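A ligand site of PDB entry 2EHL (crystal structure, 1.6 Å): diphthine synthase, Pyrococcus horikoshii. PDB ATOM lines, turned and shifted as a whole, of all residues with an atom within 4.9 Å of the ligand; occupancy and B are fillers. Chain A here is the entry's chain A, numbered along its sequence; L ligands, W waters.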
ATOM      1  N   LEU A  10       5.291  -7.534 -12.487  1.00  0.00           N
ATOM      2  CA  LEU A  10       6.614  -8.109 -12.659  1.00  0.00           C
ATOM      3  C   LEU A  10       7.904  -7.335 -12.460  1.00  0.00           C
ATOM      4  O   LEU A  10       8.845  -7.851 -11.852  1.00  0.00           O
ATOM      5  CB  LEU A  10       6.700  -8.700 -14.068  1.00  0.00           C
ATOM      6  CG  LEU A  10       5.686  -9.756 -14.489  1.00  0.00           C
ATOM      7  CD1 LEU A  10       5.670  -9.875 -16.008  1.00  0.00           C
ATOM      8  CD2 LEU A  10       6.055 -11.083 -13.844  1.00  0.00           C
ATOM      9  N   TYR A  11       7.946  -6.111 -12.971  1.00  0.00           N
ATOM     10  CA  TYR A  11       9.197  -5.374 -12.958  1.00  0.00           C
ATOM     11  C   TYR A  11       9.202  -3.931 -12.457  1.00  0.00           C
ATOM     12  O   TYR A  11      10.047  -3.570 -11.642  1.00  0.00           O
ATOM     13  CB  TYR A  11       9.751  -5.431 -14.392  1.00  0.00           C
ATOM     14  CG  TYR A  11      11.105  -4.834 -14.606  1.00  0.00           C
ATOM     15  CD1 TYR A  11      12.247  -5.446 -14.099  1.00  0.00           C
ATOM     16  CD2 TYR A  11      11.261  -3.669 -15.354  1.00  0.00           C
ATOM     17  CE1 TYR A  11      13.511  -4.916 -14.336  1.00  0.00           C
ATOM     18  CE2 TYR A  11      12.510  -3.131 -15.593  1.00  0.00           C
ATOM     19  CZ  TYR A  11      13.631  -3.755 -15.087  1.00  0.00           C
ATOM     20  OH  TYR A  11      14.872  -3.219 -15.332  1.00  0.00           O
ATOM     21  N   THR A  36       8.196 -11.098  -0.812  1.00  0.00           N
ATOM     22  CA  THR A  36       7.827 -12.275  -1.589  1.00  0.00           C
ATOM     23  C   THR A  36       8.470 -12.298  -2.968  1.00  0.00           C
ATOM     24  O   THR A  36       8.603 -13.354  -3.583  1.00  0.00           O
ATOM     25  CB  THR A  36       6.291 -12.391  -1.754  1.00  0.00           C
ATOM     26  OG1 THR A  36       5.777 -11.201  -2.359  1.00  0.00           O
ATOM     27  CG2 THR A  36       5.621 -12.602  -0.414  1.00  0.00           C
ATOM     28  N   SER A  37       8.889 -11.128  -3.452  1.00  0.00           N
ATOM     29  CA  SER A  37       9.542 -11.053  -4.750  1.00  0.00           C
ATOM     30  C   SER A  37      10.295  -9.737  -4.901  1.00  0.00           C
ATOM     31  O   SER A  37      10.252  -8.878  -4.020  1.00  0.00           O
ATOM     32  CB  SER A  37       8.508 -11.188  -5.881  1.00  0.00           C
ATOM     33  OG  SER A  37       9.162 -11.277  -7.130  1.00  0.00           O
ATOM     34  N   LEU A  38      10.992  -9.598  -6.029  1.00  0.00           N
ATOM     35  CA  LEU A  38      11.768  -8.398  -6.296  1.00  0.00           C
ATOM     36  C   LEU A  38      11.348  -7.703  -7.592  1.00  0.00           C
ATOM     37  O   LEU A  38      11.317  -8.329  -8.654  1.00  0.00           O
ATOM     38  CB  LEU A  38      13.258  -8.747  -6.388  1.00  0.00           C
ATOM     39  CG  LEU A  38      14.206  -7.641  -6.887  1.00  0.00           C
ATOM     40  CD1 LEU A  38      14.230  -6.492  -5.892  1.00  0.00           C
ATOM     41  CD2 LEU A  38      15.598  -8.216  -7.080  1.00  0.00           C
ATOM     42  N   PRO A  85       4.381  -7.390  -4.941  1.00  0.00           N
ATOM     43  CA  PRO A  85       4.990  -7.651  -6.230  1.00  0.00           C
ATOM     44  C   PRO A  85       4.185  -8.688  -7.009  1.00  0.00           C
ATOM     45  O   PRO A  85       3.524  -9.550  -6.439  1.00  0.00           O
ATOM     46  CB  PRO A  85       6.406  -8.176  -5.974  1.00  0.00           C
ATOM     47  CG  PRO A  85       6.756  -7.898  -4.511  1.00  0.00           C
ATOM     48  CD  PRO A  85       5.291  -7.720  -3.866  1.00  0.00           C
ATOM     49  N   GLY A  86       4.262  -8.670  -8.333  1.00  0.00           N
ATOM     50  CA  GLY A  86       3.565  -9.667  -9.149  1.00  0.00           C
ATOM     51  C   GLY A  86       2.095  -9.751  -8.826  1.00  0.00           C
ATOM     52  O   GLY A  86       1.434  -8.725  -8.627  1.00  0.00           O
ATOM     53  N   ASP A  87       1.559 -10.977  -8.788  1.00  0.00           N
ATOM     54  CA  ASP A  87       0.164 -11.203  -8.437  1.00  0.00           C
ATOM     55  C   ASP A  87       0.185 -11.530  -6.948  1.00  0.00           C
ATOM     56  O   ASP A  87       0.970 -12.366  -6.496  1.00  0.00           O
ATOM     57  CB  ASP A  87      -0.423 -12.365  -9.243  1.00  0.00           C
ATOM     58  CG  ASP A  87      -1.879 -12.629  -8.934  1.00  0.00           C
ATOM     59  OD1 ASP A  87      -2.182 -13.068  -7.804  1.00  0.00           O
ATOM     60  OD2 ASP A  87      -2.728 -12.371  -9.807  1.00  0.00           O
ATOM     61  N   VAL A  90      -0.087 -15.542  -5.931  1.00  0.00           N
ATOM     62  CA  VAL A  90       0.695 -16.550  -6.642  1.00  0.00           C
ATOM     63  C   VAL A  90       2.023 -16.785  -5.938  1.00  0.00           C
ATOM     64  O   VAL A  90       2.830 -15.870  -5.797  1.00  0.00           O
ATOM     65  CB  VAL A  90       0.992 -16.112  -8.097  1.00  0.00           C
ATOM     66  CG1 VAL A  90       1.914 -17.127  -8.767  1.00  0.00           C
ATOM     67  CG2 VAL A  90      -0.303 -16.004  -8.892  1.00  0.00           C
ATOM     68  N   ALA A  91       2.257 -18.020  -5.509  1.00  0.00           N
ATOM     69  CA  ALA A  91       3.504 -18.362  -4.825  1.00  0.00           C
ATOM     70  C   ALA A  91       3.723 -17.528  -3.568  1.00  0.00           C
ATOM     71  O   ALA A  91       4.833 -17.129  -3.241  1.00  0.00           O
ATOM     72  CB  ALA A  91       4.687 -18.195  -5.783  1.00  0.00           C
ATOM     73  N   THR A  92       2.612 -17.236  -2.886  1.00  0.00           N
ATOM     74  CA  THR A  92       2.614 -16.551  -1.610  1.00  0.00           C
ATOM     75  C   THR A  92       1.587 -17.265  -0.783  1.00  0.00           C
ATOM     76  O   THR A  92       0.910 -18.168  -1.244  1.00  0.00           O
ATOM     77  CB  THR A  92       2.188 -15.068  -1.777  1.00  0.00           C
ATOM     78  OG1 THR A  92       0.779 -14.977  -1.986  1.00  0.00           O
ATOM     79  CG2 THR A  92       2.923 -14.382  -2.938  1.00  0.00           C
ATOM     80  N   PRO A 114       0.288  -8.898 -13.657  1.00  0.00           N
ATOM     81  CA  PRO A 114       1.091  -9.931 -14.318  1.00  0.00           C
ATOM     82  C   PRO A 114       1.979 -10.685 -13.330  1.00  0.00           C
ATOM     83  O   PRO A 114       2.611 -10.085 -12.456  1.00  0.00           O
ATOM     84  CB  PRO A 114       1.867  -9.151 -15.386  1.00  0.00           C
ATOM     85  CG  PRO A 114       1.709  -7.678 -15.123  1.00  0.00           C
ATOM     86  CD  PRO A 114       0.484  -7.580 -14.284  1.00  0.00           C
ATOM     87  N   SER A 115       2.004 -12.008 -13.499  1.00  0.00           N
ATOM     88  CA  SER A 115       2.752 -12.912 -12.624  1.00  0.00           C
ATOM     89  C   SER A 115       3.831 -13.686 -13.373  1.00  0.00           C
ATOM     90  O   SER A 115       3.673 -14.018 -14.541  1.00  0.00           O
ATOM     91  CB  SER A 115       1.771 -13.895 -11.980  1.00  0.00           C
ATOM     92  OG  SER A 115       2.449 -14.933 -11.295  1.00  0.00           O
ATOM     93  N   ILE A 116       4.921 -14.008 -12.681  1.00  0.00           N
ATOM     94  CA  ILE A 116       5.998 -14.765 -13.301  1.00  0.00           C
ATOM     95  C   ILE A 116       5.495 -16.149 -13.708  1.00  0.00           C
ATOM     96  O   ILE A 116       5.986 -16.741 -14.665  1.00  0.00           O
ATOM     97  CB  ILE A 116       7.220 -14.893 -12.338  1.00  0.00           C
ATOM     98  CG1 ILE A 116       8.405 -15.510 -13.085  1.00  0.00           C
ATOM     99  CG2 ILE A 116       6.855 -15.766 -11.140  1.00  0.00           C
ATOM    100  CD1 ILE A 116       8.889 -14.671 -14.254  1.00  0.00           C
ATOM    101  N   TYR A 117       4.504 -16.648 -12.979  1.00  0.00           N
ATOM    102  CA  TYR A 117       3.927 -17.964 -13.236  1.00  0.00           C
ATOM    103  C   TYR A 117       3.380 -18.081 -14.662  1.00  0.00           C
ATOM    104  O   TYR A 117       3.476 -19.145 -15.294  1.00  0.00           O
ATOM    105  CB  TYR A 117       2.837 -18.256 -12.197  1.00  0.00           C
ATOM    106  CG  TYR A 117       2.157 -19.601 -12.310  1.00  0.00           C
ATOM    107  CD1 TYR A 117       2.849 -20.797 -12.097  1.00  0.00           C
ATOM    108  CD2 TYR A 117       0.791 -19.674 -12.592  1.00  0.00           C
ATOM    109  CE1 TYR A 117       2.189 -22.023 -12.167  1.00  0.00           C
ATOM    110  CE2 TYR A 117       0.132 -20.896 -12.648  1.00  0.00           C
ATOM    111  CZ  TYR A 117       0.830 -22.061 -12.438  1.00  0.00           C
ATOM    112  OH  TYR A 117       0.148 -23.263 -12.490  1.00  0.00           O
ATOM    113  N   PHE A 165      10.853 -21.604  -8.961  1.00  0.00           N
ATOM    114  CA  PHE A 165      10.908 -20.295  -8.320  1.00  0.00           C
ATOM    115  C   PHE A 165      12.231 -20.316  -7.561  1.00  0.00           C
ATOM    116  O   PHE A 165      12.590 -21.352  -6.988  1.00  0.00           O
ATOM    117  CB  PHE A 165       9.768 -20.131  -7.316  1.00  0.00           C
ATOM    118  CG  PHE A 165       8.401 -20.053  -7.940  1.00  0.00           C
ATOM    119  CD1 PHE A 165       7.930 -18.857  -8.469  1.00  0.00           C
ATOM    120  CD2 PHE A 165       7.575 -21.178  -7.972  1.00  0.00           C
ATOM    121  CE1 PHE A 165       6.649 -18.782  -9.019  1.00  0.00           C
ATOM    122  CE2 PHE A 165       6.288 -21.110  -8.511  1.00  0.00           C
ATOM    123  CZ  PHE A 165       5.838 -19.902  -9.039  1.00  0.00           C
ATOM    124  N   LEU A 166      12.949 -19.203  -7.538  1.00  0.00           N
ATOM    125  CA  LEU A 166      14.220 -19.162  -6.837  1.00  0.00           C
ATOM    126  C   LEU A 166      14.093 -18.414  -5.523  1.00  0.00           C
ATOM    127  O   LEU A 166      13.289 -17.491  -5.384  1.00  0.00           O
ATOM    128  CB  LEU A 166      15.301 -18.545  -7.728  1.00  0.00           C
ATOM    129  CG  LEU A 166      15.446 -19.298  -9.065  1.00  0.00           C
ATOM    130  CD1 LEU A 166      16.612 -18.730  -9.860  1.00  0.00           C
ATOM    131  CD2 LEU A 166      15.640 -20.797  -8.812  1.00  0.00           C
ATOM    132  N   ASP A 167      14.891 -18.823  -4.540  1.00  0.00           N
ATOM    133  CA  ASP A 167      14.823 -18.225  -3.223  1.00  0.00           C
ATOM    134  C   ASP A 167      15.148 -16.738  -3.164  1.00  0.00           C
ATOM    135  O   ASP A 167      15.822 -16.194  -4.041  1.00  0.00           O
ATOM    136  CB  ASP A 167      15.745 -18.971  -2.248  1.00  0.00           C
ATOM    137  CG  ASP A 167      15.174 -19.038  -0.842  1.00  0.00           C
ATOM    138  OD1 ASP A 167      14.206 -18.324  -0.544  1.00  0.00           O
ATOM    139  OD2 ASP A 167      15.717 -19.819  -0.021  1.00  0.00           O
ATOM    140  N   ILE A 168      14.641 -16.093  -2.126  1.00  0.00           N
ATOM    141  CA  ILE A 168      14.852 -14.684  -1.907  1.00  0.00           C
ATOM    142  C   ILE A 168      14.835 -14.406  -0.410  1.00  0.00           C
ATOM    143  O   ILE A 168      14.011 -14.952   0.325  1.00  0.00           O
ATOM    144  CB  ILE A 168      13.757 -13.826  -2.589  1.00  0.00           C
ATOM    145  CG1 ILE A 168      13.850 -12.375  -2.120  1.00  0.00           C
ATOM    146  CG2 ILE A 168      12.376 -14.408  -2.280  1.00  0.00           C
ATOM    147  CD1 ILE A 168      12.847 -11.437  -2.767  1.00  0.00           C
ATOM    148  N   LEU A 206      14.964 -17.238 -17.386  1.00  0.00           N
ATOM    149  CA  LEU A 206      14.213 -16.025 -17.665  1.00  0.00           C
ATOM    150  C   LEU A 206      14.566 -15.053 -16.551  1.00  0.00           C
ATOM    151  O   LEU A 206      14.316 -15.327 -15.372  1.00  0.00           O
ATOM    152  CB  LEU A 206      12.701 -16.295 -17.683  1.00  0.00           C
ATOM    153  CG  LEU A 206      11.797 -15.064 -17.857  1.00  0.00           C
ATOM    154  CD1 LEU A 206      12.153 -14.330 -19.139  1.00  0.00           C
ATOM    155  CD2 LEU A 206      10.330 -15.509 -17.878  1.00  0.00           C
ATOM    156  N   ALA A 207      15.149 -13.918 -16.914  1.00  0.00           N
ATOM    157  CA  ALA A 207      15.544 -12.928 -15.928  1.00  0.00           C
ATOM    158  C   ALA A 207      14.901 -11.578 -16.198  1.00  0.00           C
ATOM    159  O   ALA A 207      14.896 -11.091 -17.322  1.00  0.00           O
ATOM    160  CB  ALA A 207      17.067 -12.777 -15.928  1.00  0.00           C
ATOM    161  N   ARG A 208      14.356 -10.982 -15.141  1.00  0.00           N
ATOM    162  CA  ARG A 208      13.695  -9.691 -15.214  1.00  0.00           C
ATOM    163  C   ARG A 208      12.514  -9.664 -16.174  1.00  0.00           C
ATOM    164  O   ARG A 208      12.395  -8.773 -17.029  1.00  0.00           O
ATOM    165  CB  ARG A 208      14.722  -8.615 -15.586  1.00  0.00           C
ATOM    166  CG  ARG A 208      15.892  -8.542 -14.604  1.00  0.00           C
ATOM    167  CD  ARG A 208      16.915  -7.491 -15.027  1.00  0.00           C
ATOM    168  NE  ARG A 208      17.294  -7.667 -16.424  1.00  0.00           N
ATOM    169  CZ  ARG A 208      18.038  -8.669 -16.890  1.00  0.00           C
ATOM    170  NH1 ARG A 208      18.506  -9.600 -16.061  1.00  0.00           N
ATOM    171  NH2 ARG A 208      18.295  -8.753 -18.185  1.00  0.00           N
ATOM    172  N   ALA A 209      11.633 -10.655 -16.056  1.00  0.00           N
ATOM    173  CA  ALA A 209      10.441 -10.687 -16.892  1.00  0.00           C
ATOM    174  C   ALA A 209       9.686  -9.406 -16.576  1.00  0.00           C
ATOM    175  O   ALA A 209       9.718  -8.916 -15.444  1.00  0.00           O
ATOM    176  CB  ALA A 209       9.597 -11.912 -16.545  1.00  0.00           C
ATOM    177  N   GLY A 210       9.014  -8.846 -17.579  1.00  0.00           N
ATOM    178  CA  GLY A 210       8.282  -7.616 -17.338  1.00  0.00           C
ATOM    179  C   GLY A 210       9.033  -6.421 -17.905  1.00  0.00           C
ATOM    180  O   GLY A 210       8.431  -5.428 -18.303  1.00  0.00           O
ATOM    181  N   PRO A 233      15.431 -10.308 -10.522  1.00  0.00           N
ATOM    182  CA  PRO A 233      15.169 -11.718 -10.224  1.00  0.00           C
ATOM    183  C   PRO A 233      15.309 -12.643 -11.435  1.00  0.00           C
ATOM    184  O   PRO A 233      15.190 -12.216 -12.589  1.00  0.00           O
ATOM    185  CB  PRO A 233      13.751 -11.681  -9.683  1.00  0.00           C
ATOM    186  CG  PRO A 233      13.118 -10.638 -10.544  1.00  0.00           C
ATOM    187  CD  PRO A 233      14.166  -9.546 -10.582  1.00  0.00           C
ATOM    188  N   HIS A 234      15.559 -13.917 -11.144  1.00  0.00           N
ATOM    189  CA  HIS A 234      15.690 -14.955 -12.164  1.00  0.00           C
ATOM    190  C   HIS A 234      14.772 -16.099 -11.804  1.00  0.00           C
ATOM    191  O   HIS A 234      14.387 -16.274 -10.642  1.00  0.00           O
ATOM    192  CB  HIS A 234      17.083 -15.580 -12.172  1.00  0.00           C
ATOM    193  CG  HIS A 234      18.208 -14.639 -12.497  1.00  0.00           C
ATOM    194  ND1 HIS A 234      19.520 -15.047 -12.489  1.00  0.00           N
ATOM    195  CD2 HIS A 234      18.213 -13.329 -12.845  1.00  0.00           C
ATOM    196  CE1 HIS A 234      20.297 -14.022 -12.822  1.00  0.00           C
ATOM    197  NE2 HIS A 234      19.526 -12.971 -13.043  1.00  0.00           N
ATOM    198  N   ILE A 235      14.421 -16.892 -12.809  1.00  0.00           N
ATOM    199  CA  ILE A 235      13.638 -18.094 -12.615  1.00  0.00           C
ATOM    200  C   ILE A 235      14.333 -19.134 -13.487  1.00  0.00           C
ATOM    201  O   ILE A 235      14.908 -18.792 -14.524  1.00  0.00           O
ATOM    202  CB  ILE A 235      12.159 -17.947 -13.042  1.00  0.00           C
ATOM    203  CG1 ILE A 235      11.307 -18.955 -12.269  1.00  0.00           C
ATOM    204  CG2 ILE A 235      12.007 -18.135 -14.542  1.00  0.00           C
ATOM    205  CD1 ILE A 235      10.008 -18.380 -11.744  1.00  0.00           C
HETATM  206  N1  LIG L   1       3.548 -13.418  -6.559  1.00  0.00           N
HETATM  207  C1  LIG L   1       4.792 -13.377  -7.426  1.00  0.00           C
HETATM  208  C2  LIG L   1       5.782 -14.483  -7.246  1.00  0.00           C
HETATM  209  C3  LIG L   1       6.364 -14.687  -5.853  1.00  0.00           C
HETATM  210  S1  LIG L   1       7.712 -15.928  -5.991  1.00  0.00           S
HETATM  211  C4  LIG L   1       4.284 -13.327  -8.936  1.00  0.00           C
HETATM  212  O1  LIG L   1       3.065 -13.349  -9.158  1.00  0.00           O
HETATM  213  O2  LIG L   1       5.200 -13.253  -9.850  1.00  0.00           O
HETATM  214  C5  LIG L   1       9.069 -14.862  -6.279  1.00  0.00           C
HETATM  215  C6  LIG L   1      10.146 -15.553  -7.208  1.00  0.00           C
HETATM  216  O3  LIG L   1       9.572 -15.622  -8.535  1.00  0.00           O
HETATM  217  C7  LIG L   1      11.432 -14.822  -7.338  1.00  0.00           C
HETATM  218  O4  LIG L   1      12.339 -15.197  -6.309  1.00  0.00           O
HETATM  219  C8  LIG L   1      11.861 -15.225  -8.775  1.00  0.00           C
HETATM  220  O5  LIG L   1      12.510 -16.506  -8.808  1.00  0.00           O
HETATM  221  C9  LIG L   1      10.555 -15.203  -9.573  1.00  0.00           C
HETATM  222  N2  LIG L   1      10.199 -14.007 -10.098  1.00  0.00           N
HETATM  223  C10 LIG L   1       9.302 -13.016  -9.734  1.00  0.00           C
HETATM  224  N3  LIG L   1       9.246 -12.000 -10.537  1.00  0.00           N
HETATM  225  C11 LIG L   1      10.178 -12.301 -11.555  1.00  0.00           C
HETATM  226  C12 LIG L   1      10.567 -11.578 -12.740  1.00  0.00           C
HETATM  227  N4  LIG L   1      10.052 -10.384 -13.080  1.00  0.00           N
HETATM  228  N5  LIG L   1      11.521 -12.192 -13.511  1.00  0.00           N
HETATM  229  C13 LIG L   1      12.075 -13.402 -13.200  1.00  0.00           C
HETATM  230  N6  LIG L   1      11.714 -14.122 -12.085  1.00  0.00           N
HETATM  231  C14 LIG L   1      10.775 -13.517 -11.313  1.00  0.00           C
HETATM  232  O   HOH W   1       6.715 -10.739 -10.200  1.00  0.00           O
HETATM  233  O   HOH W   2       4.630 -11.530  -4.770  1.00  0.00           O
HETATM  234  O   HOH W   3      14.951 -14.226  -6.106  1.00  0.00           O
HETATM  235  O   HOH W   4       8.272  -9.220  -8.671  1.00  0.00           O
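The backbone carbonyl oxygen (O) of Leu 10 sits at hydrogen-bond distance from a nitrogen (N4) of the ligand, at 3.1 Å. N of Ala 209 sits at hydrogen-bond distance from N5 of the ligand (3.0 Å). The side-chain hydroxyl (OG) of Ser 115 sits at hydrogen-bond distance from an oxygen (O1) of the ligand. N of Leu 166 sits at hydrogen-bond distance from O5 of the ligand. N1 of the ligand is in hydrogen-bond range of O of Asp 87, 2.8 Å away. N of Asp 87 sits at hydrogen-bond distance from O1 of the ligand. An oxygen (O4) of the ligand lies within hydrogen-bond range of the backbone carbonyl oxygen (O) of Leu 166, at 2.6 Å. The side-chain hydroxyl (OG) of Ser 37 sits close to a nitrogen (N3) of the ligand (3.5 Å). N of Ile 116 is in hydrogen-bond range of O2 of the ligand (2.9 Å). The backbone NH of Arg 208 is in hydrogen-bond range of a nitrogen (N5) of the ligand (3.5 Å). The backbone carbonyl oxygen of Val 90 is in hydrogen-bond range of a nitrogen (N1) of the ligand (2.7 Å). The backbone carbonyl oxygen (O) of Ala 209 sits at hydrogen-bond distance from a nitrogen (N4) of the ligand (2.8 Å). The backbone carbonyl oxygen (O) of His 234 lies within hydrogen-bond range of an oxygen (O5) of the ligand (2.6 Å).
Water W3 lies within hydrogen-bond range of an oxygen (O4) of the ligand (2.8 Å) and the backbone carbonyl oxygen (O) of Asp 167 (3.0 Å). Water W2 lies within hydrogen-bond range of OG1 of Thr 36, O of Pro 85 and N1 of the ligand. Water W4 lies within hydrogen-bond range of the side-chain hydroxyl of Ser 37, the backbone carbonyl oxygen of Leu 38 and a nitrogen (N3) of the ligand.
O of Thr 36 lies close to S1 of the ligand, at 3.6 Å. O of Pro 85 touches N1 of the ligand, at 3.9 Å. Gly 86 touches the ligand. CB of Ala 91 touches S1 of the ligand (3.8 Å). CG2 of Thr 92 touches N1 of the ligand, at 3.8 Å. CD1 of Phe 165 touches O3 of the ligand (3.6 Å). Leu 206 touches the ligand (O to C13, 3.7 Å). O of Pro 233 touches C13 of the ligand, at 3.4 Å. CD1 of Ile 235 touches C9 of the ligand, at 3.9 Å. Of the 27 residues printed, 19 come within 4 Å of the ligand. Along chain A the residues within 4 Å of the ligand span positions 10 to 235.
N of Ile 235 sits at hydrogen-bond distance from O of Leu 206, 3.0 Å away. The backbone carbonyl oxygen (O) of Pro 233 lies within hydrogen-bond range of the backbone NH (N) of Arg 208. The side-chain hydroxyl (OG) of Ser 115 sits close to the backbone NH (N) of Tyr 117, at 3.2 Å.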
